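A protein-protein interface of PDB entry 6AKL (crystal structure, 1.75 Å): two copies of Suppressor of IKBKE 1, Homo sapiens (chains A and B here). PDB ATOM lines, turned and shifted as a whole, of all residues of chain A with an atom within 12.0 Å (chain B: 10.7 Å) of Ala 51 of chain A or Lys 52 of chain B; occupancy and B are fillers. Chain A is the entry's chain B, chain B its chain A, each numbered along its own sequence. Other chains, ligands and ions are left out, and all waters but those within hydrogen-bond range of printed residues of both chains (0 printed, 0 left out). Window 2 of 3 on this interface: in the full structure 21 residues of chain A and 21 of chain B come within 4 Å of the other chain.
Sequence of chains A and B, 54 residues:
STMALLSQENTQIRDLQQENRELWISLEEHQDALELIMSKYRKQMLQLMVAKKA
Printed residues of chain A that touch a printed residue of chain B: Gln 44, Met 45, Gln 47, Leu 48 and Ala 51. Hydrophobic or aromatic side chains of chain A that line the printed part of chain B: Met 45, Leu 48 and Ala 51. Printed residues of chain B that touch a printed residue of chain A: Gln 44, Met 45, Gln 47, Leu 48 and Lys 52. Among the printed residues, 8 pairs touch across the chains.
Gln 44 of chain A touches its own counterpart, Gln 44 of chain B. Gln 44 of chain A touches Met 45 of chain B, and with the chains exchanged Met 45 of chain A touches Gln 44 of chain B. Gln 44 of chain A touches Leu 48 of chain B, but with the chains exchanged Leu 48 of chain A does not touch Gln 44 of chain B (4.1 Å). Ala 51 of chain A touches Lys 52 of chain B, but with the chains exchanged Lys 52 of chain A does not touch Ala 51 of chain B (4.3 Å). 9 positions are printed for both chains.
The side-chain amide oxygen (OE1) of Gln 44 of chain B is in hydrogen-bond range of the backbone NH (N) of Met 45 of chain A, at 3.4 Å. The side-chain amide oxygen (OE1) of Gln 44 of chain B lies within hydrogen-bond range of the side-chain amide nitrogen (NE2) of Gln 44 of chain A (2.8 Å).
Among the printed residues, merely in contact across the chains: Gln 44 of chain A with Met 45 of chain B (3.2 Å), Gln 44 of chain A with Leu 48 of chain B (3.8 Å), Gln 47 of chain A with Leu 48 of chain B (3.7 Å), Leu 48 of chain A with Gln 47 of chain B (3.5 Å), Leu 48 of chain A with Leu 48 of chain B (3.7 Å) and Ala 51 of chain A with Lys 52 of chain B (3.7 Å).
Printed residues of chain B within 4 Å of Gln 44 of chain A: Gln 44 (2.8 Å), Met 45 (3.2 Å) and Leu 48 (3.8 Å). Of the printed residues of chain B, Met 45 of chain A touches Gln 44 (3.3 Å). Of the printed residues of chain B, Gln 47 of chain A touches Leu 48 (3.7 Å). Of the printed residues of chain B, Leu 48 of chain A touches Gln 47 (3.5 Å) and Leu 48 (3.7 Å). No residue of chain B comes within 4 Å of Val 50 of chain A. Of the printed residues of chain A, Gln 44 of chain B touches Gln 44 and Met 45. Of the printed residues of chain A, Gln 47 of chain B touches Leu 48 (3.5 Å). Of chain A, only Gln 44, Gln 47 and Leu 48 come within 4 Å of Leu 48 of chain B. No residue of chain A comes within 4 Å of Met 49 of chain B. No residue of chain A comes within 4 Å of Ala 51 of chain B. Of chain A, only Ala 51 (3.7 Å) comes within 4 Å of Lys 52 of chain B. The nearest residue of chain B that does not touch Ala 51 of chain A is Leu 48 of chain B (4.2 Å).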
ATOM      1  N   ARG A  42       6.534  15.611  18.526  1.00  0.00           N
ATOM      2  CA  ARG A  42       6.401  14.176  18.318  1.00  0.00           C
ATOM      3  C   ARG A  42       7.502  13.653  17.407  1.00  0.00           C
ATOM      4  O   ARG A  42       8.135  12.635  17.704  1.00  0.00           O
ATOM      5  CB  ARG A  42       5.027  13.865  17.727  1.00  0.00           C
ATOM      6  CG  ARG A  42       4.744  12.396  17.606  1.00  0.00           C
ATOM      7  CD  ARG A  42       3.430  12.138  16.856  1.00  0.00           C
ATOM      8  NE  ARG A  42       3.339  12.785  15.537  1.00  0.00           N
ATOM      9  CZ  ARG A  42       3.974  12.356  14.442  1.00  0.00           C
ATOM     10  NH1 ARG A  42       4.778  11.307  14.503  1.00  0.00           N
ATOM     11  NH2 ARG A  42       3.828  12.989  13.286  1.00  0.00           N
ATOM     12  N   LYS A  43       7.747  14.343  16.290  1.00  0.00           N
ATOM     13  CA  LYS A  43       8.781  13.890  15.369  1.00  0.00           C
ATOM     14  C   LYS A  43      10.173  13.979  15.983  1.00  0.00           C
ATOM     15  O   LYS A  43      11.047  13.162  15.658  1.00  0.00           O
ATOM     16  CB  LYS A  43       8.712  14.698  14.080  1.00  0.00           C
ATOM     17  CG  LYS A  43       7.462  14.391  13.281  1.00  0.00           C
ATOM     18  CD  LYS A  43       7.613  14.801  11.840  1.00  0.00           C
ATOM     19  CE  LYS A  43       6.484  15.699  11.410  1.00  0.00           C
ATOM     20  NZ  LYS A  43       5.547  14.960  10.518  1.00  0.00           N
ATOM     21  N   GLN A  44      10.406  14.962  16.857  1.00  0.00           N
ATOM     22  CA  GLN A  44      11.676  15.023  17.579  1.00  0.00           C
ATOM     23  C   GLN A  44      11.820  13.835  18.519  1.00  0.00           C
ATOM     24  O   GLN A  44      12.921  13.287  18.685  1.00  0.00           O
ATOM     25  CB  GLN A  44      11.781  16.339  18.363  1.00  0.00           C
ATOM     26  CG  GLN A  44      13.099  16.495  19.131  1.00  0.00           C
ATOM     27  CD  GLN A  44      13.214  17.832  19.858  1.00  0.00           C
ATOM     28  OE1 GLN A  44      14.128  18.619  19.592  1.00  0.00           O
ATOM     29  NE2 GLN A  44      12.293  18.087  20.786  1.00  0.00           N
ATOM     30  N   MET A  45      10.722  13.426  19.154  1.00  0.00           N
ATOM     31  CA  MET A  45      10.783  12.252  20.015  1.00  0.00           C
ATOM     32  C   MET A  45      11.140  11.008  19.212  1.00  0.00           C
ATOM     33  O   MET A  45      11.920  10.163  19.673  1.00  0.00           O
ATOM     34  CB  MET A  45       9.451  12.072  20.741  1.00  0.00           C
ATOM     35  CG  MET A  45       9.528  11.225  21.990  1.00  0.00           C
ATOM     36  SD  MET A  45       7.968  11.257  22.891  1.00  0.00           S
ATOM     37  CE  MET A  45       8.078  12.839  23.730  1.00  0.00           C
ATOM     38  N   LEU A  46      10.586  10.885  17.999  1.00  0.00           N
ATOM     39  CA  LEU A  46      10.939   9.775  17.116  1.00  0.00           C
ATOM     40  C   LEU A  46      12.428   9.781  16.803  1.00  0.00           C
ATOM     41  O   LEU A  46      13.088   8.734  16.830  1.00  0.00           O
ATOM     42  CB  LEU A  46      10.122   9.847  15.822  1.00  0.00           C
ATOM     43  CG  LEU A  46       8.706   9.268  15.873  1.00  0.00           C
ATOM     44  CD1 LEU A  46       7.895   9.623  14.617  1.00  0.00           C
ATOM     45  CD2 LEU A  46       8.759   7.761  16.068  1.00  0.00           C
ATOM     46  N   GLN A  47      12.978  10.956  16.501  1.00  0.00           N
ATOM     47  CA  GLN A  47      14.403  11.015  16.208  1.00  0.00           C
ATOM     48  C   GLN A  47      15.239  10.729  17.451  1.00  0.00           C
ATOM     49  O   GLN A  47      16.325  10.144  17.344  1.00  0.00           O
ATOM     50  CB  GLN A  47      14.766  12.368  15.597  1.00  0.00           C
ATOM     51  CG  GLN A  47      16.260  12.523  15.348  1.00  0.00           C
ATOM     52  CD  GLN A  47      16.803  11.440  14.423  1.00  0.00           C
ATOM     53  OE1 GLN A  47      17.889  10.896  14.645  1.00  0.00           O
ATOM     54  NE2 GLN A  47      16.041  11.120  13.380  1.00  0.00           N
ATOM     55  N   LEU A  48      14.754  11.108  18.638  1.00  0.00           N
ATOM     56  CA  LEU A  48      15.471  10.724  19.854  1.00  0.00           C
ATOM     57  C   LEU A  48      15.395   9.221  20.087  1.00  0.00           C
ATOM     58  O   LEU A  48      16.316   8.632  20.668  1.00  0.00           O
ATOM     59  CB  LEU A  48      14.925  11.482  21.064  1.00  0.00           C
ATOM     60  CG  LEU A  48      15.695  11.298  22.378  1.00  0.00           C
ATOM     61  CD1 LEU A  48      17.129  11.816  22.262  1.00  0.00           C
ATOM     62  CD2 LEU A  48      14.980  11.986  23.529  1.00  0.00           C
ATOM     63  N   MET A  49      14.310   8.589  19.634  1.00  0.00           N
ATOM     64  CA  MET A  49      14.191   7.139  19.727  1.00  0.00           C
ATOM     65  C   MET A  49      15.140   6.449  18.753  1.00  0.00           C
ATOM     66  O   MET A  49      15.719   5.404  19.074  1.00  0.00           O
ATOM     67  CB  MET A  49      12.740   6.733  19.461  1.00  0.00           C
ATOM     68  CG  MET A  49      12.469   5.240  19.439  1.00  0.00           C
ATOM     69  SD  MET A  49      10.748   4.916  19.878  1.00  0.00           S
ATOM     70  CE  MET A  49      10.574   3.199  19.415  1.00  0.00           C
ATOM     71  N   VAL A  50      15.319   7.030  17.564  1.00  0.00           N
ATOM     72  CA  VAL A  50      16.235   6.468  16.577  1.00  0.00           C
ATOM     73  C   VAL A  50      17.680   6.596  17.050  1.00  0.00           C
ATOM     74  O   VAL A  50      18.484   5.667  16.899  1.00  0.00           O
ATOM     75  CB  VAL A  50      16.015   7.154  15.215  1.00  0.00           C
ATOM     76  CG1 VAL A  50      17.273   7.101  14.363  1.00  0.00           C
ATOM     77  CG2 VAL A  50      14.810   6.540  14.484  1.00  0.00           C
ATOM     78  N   ALA A  51      18.029   7.739  17.647  1.00  0.00           N
ATOM     79  CA  ALA A  51      19.403   7.959  18.087  1.00  0.00           C
ATOM     80  C   ALA A  51      19.741   7.116  19.313  1.00  0.00           C
ATOM     81  O   ALA A  51      20.834   6.542  19.394  1.00  0.00           O
ATOM     82  CB  ALA A  51      19.633   9.443  18.373  1.00  0.00           C
ATOM     83  N   LYS A  52      18.828   7.032  20.275  1.00  0.00           N
ATOM     84  CA  LYS A  52      19.064   6.221  21.466  1.00  0.00           C
ATOM     85  C   LYS A  52      18.764   4.748  21.197  1.00  0.00           C
ATOM     86  O   LYS A  52      19.256   4.168  20.226  1.00  0.00           O
ATOM     87  CB  LYS A  52      18.220   6.720  22.640  1.00  0.00           C
ATOM     88  CG  LYS A  52      18.696   8.032  23.235  1.00  0.00           C
ATOM     89  CD  LYS A  52      18.051   8.279  24.586  1.00  0.00           C
ATOM     90  N   GLN B  44      14.181  18.047  25.270  1.00  0.00           N
ATOM     91  CA  GLN B  44      14.379  16.909  24.376  1.00  0.00           C
ATOM     92  C   GLN B  44      15.427  17.213  23.310  1.00  0.00           C
ATOM     93  O   GLN B  44      16.197  16.323  22.921  1.00  0.00           O
ATOM     94  CB  GLN B  44      13.024  16.532  23.767  1.00  0.00           C
ATOM     95  CG  GLN B  44      12.997  15.467  22.694  1.00  0.00           C
ATOM     96  CD  GLN B  44      11.557  15.112  22.317  1.00  0.00           C
ATOM     97  OE1 GLN B  44      10.887  15.837  21.555  1.00  0.00           O
ATOM     98  NE2 GLN B  44      11.064  14.011  22.874  1.00  0.00           N
ATOM     99  N   MET B  45      15.507  18.471  22.866  1.00  0.00           N
ATOM    100  CA  MET B  45      16.501  18.856  21.868  1.00  0.00           C
ATOM    101  C   MET B  45      17.916  18.761  22.425  1.00  0.00           C
ATOM    102  O   MET B  45      18.853  18.402  21.703  1.00  0.00           O
ATOM    103  CB  MET B  45      16.215  20.273  21.375  1.00  0.00           C
ATOM    104  CG  MET B  45      17.358  20.922  20.634  1.00  0.00           C
ATOM    105  SD  MET B  45      16.769  22.045  19.354  1.00  0.00           S
ATOM    106  CE  MET B  45      16.191  20.873  18.121  1.00  0.00           C
ATOM    107  N   LEU B  46      18.093  19.098  23.703  1.00  0.00           N
ATOM    108  CA  LEU B  46      19.395  18.898  24.337  1.00  0.00           C
ATOM    109  C   LEU B  46      19.759  17.418  24.391  1.00  0.00           C
ATOM    110  O   LEU B  46      20.902  17.038  24.103  1.00  0.00           O
ATOM    111  CB  LEU B  46      19.402  19.504  25.739  1.00  0.00           C
ATOM    112  CG  LEU B  46      19.434  21.030  25.779  1.00  0.00           C
ATOM    113  CD1 LEU B  46      19.367  21.522  27.217  1.00  0.00           C
ATOM    114  CD2 LEU B  46      20.674  21.567  25.070  1.00  0.00           C
ATOM    115  N   GLN B  47      18.803  16.565  24.770  1.00  0.00           N
ATOM    116  CA  GLN B  47      19.076  15.130  24.782  1.00  0.00           C
ATOM    117  C   GLN B  47      19.401  14.617  23.384  1.00  0.00           C
ATOM    118  O   GLN B  47      20.277  13.758  23.216  1.00  0.00           O
ATOM    119  CB  GLN B  47      17.890  14.367  25.366  1.00  0.00           C
ATOM    120  CG  GLN B  47      17.539  14.760  26.787  1.00  0.00           C
ATOM    121  CD  GLN B  47      16.049  14.697  27.054  1.00  0.00           C
ATOM    122  OE1 GLN B  47      15.312  13.981  26.372  1.00  0.00           O
ATOM    123  NE2 GLN B  47      15.594  15.453  28.049  1.00  0.00           N
ATOM    124  N   LEU B  48      18.709  15.139  22.369  1.00  0.00           N
ATOM    125  CA  LEU B  48      18.949  14.716  20.992  1.00  0.00           C
ATOM    126  C   LEU B  48      20.348  15.110  20.525  1.00  0.00           C
ATOM    127  O   LEU B  48      21.095  14.277  20.001  1.00  0.00           O
ATOM    128  CB  LEU B  48      17.878  15.316  20.078  1.00  0.00           C
ATOM    129  CG  LEU B  48      17.816  14.823  18.637  1.00  0.00           C
ATOM    130  CD1 LEU B  48      17.912  13.308  18.597  1.00  0.00           C
ATOM    131  CD2 LEU B  48      16.539  15.308  17.965  1.00  0.00           C
ATOM    132  N   MET B  49      20.719  16.381  20.705  1.00  0.00           N
ATOM    133  CA  MET B  49      22.052  16.825  20.317  1.00  0.00           C
ATOM    134  C   MET B  49      23.144  16.171  21.154  1.00  0.00           C
ATOM    135  O   MET B  49      24.294  16.104  20.707  1.00  0.00           O
ATOM    136  CB  MET B  49      22.153  18.348  20.424  1.00  0.00           C
ATOM    137  N   VAL B  50      22.811  15.692  22.354  1.00  0.00           N
ATOM    138  CA  VAL B  50      23.785  14.995  23.187  1.00  0.00           C
ATOM    139  C   VAL B  50      24.030  13.587  22.661  1.00  0.00           C
ATOM    140  O   VAL B  50      25.179  13.147  22.531  1.00  0.00           O
ATOM    141  CB  VAL B  50      23.315  14.986  24.656  1.00  0.00           C
ATOM    142  CG1 VAL B  50      23.869  13.782  25.402  1.00  0.00           C
ATOM    143  CG2 VAL B  50      23.727  16.282  25.352  1.00  0.00           C
ATOM    144  N   ALA B  51      22.957  12.860  22.341  1.00  0.00           N
ATOM    145  CA  ALA B  51      23.112  11.518  21.791  1.00  0.00           C
ATOM    146  C   ALA B  51      23.532  11.554  20.326  1.00  0.00           C
ATOM    147  O   ALA B  51      24.410  10.789  19.913  1.00  0.00           O
ATOM    148  CB  ALA B  51      21.813  10.730  21.956  1.00  0.00           C
ATOM    149  N   LYS B  52      22.933  12.439  19.535  1.00  0.00           N
ATOM    150  CA  LYS B  52      23.192  12.489  18.098  1.00  0.00           C
ATOM    151  C   LYS B  52      23.777  13.831  17.677  1.00  0.00           C
ATOM    152  O   LYS B  52      23.515  14.307  16.571  1.00  0.00           O
ATOM    153  CB  LYS B  52      21.910  12.207  17.320  1.00  0.00           C
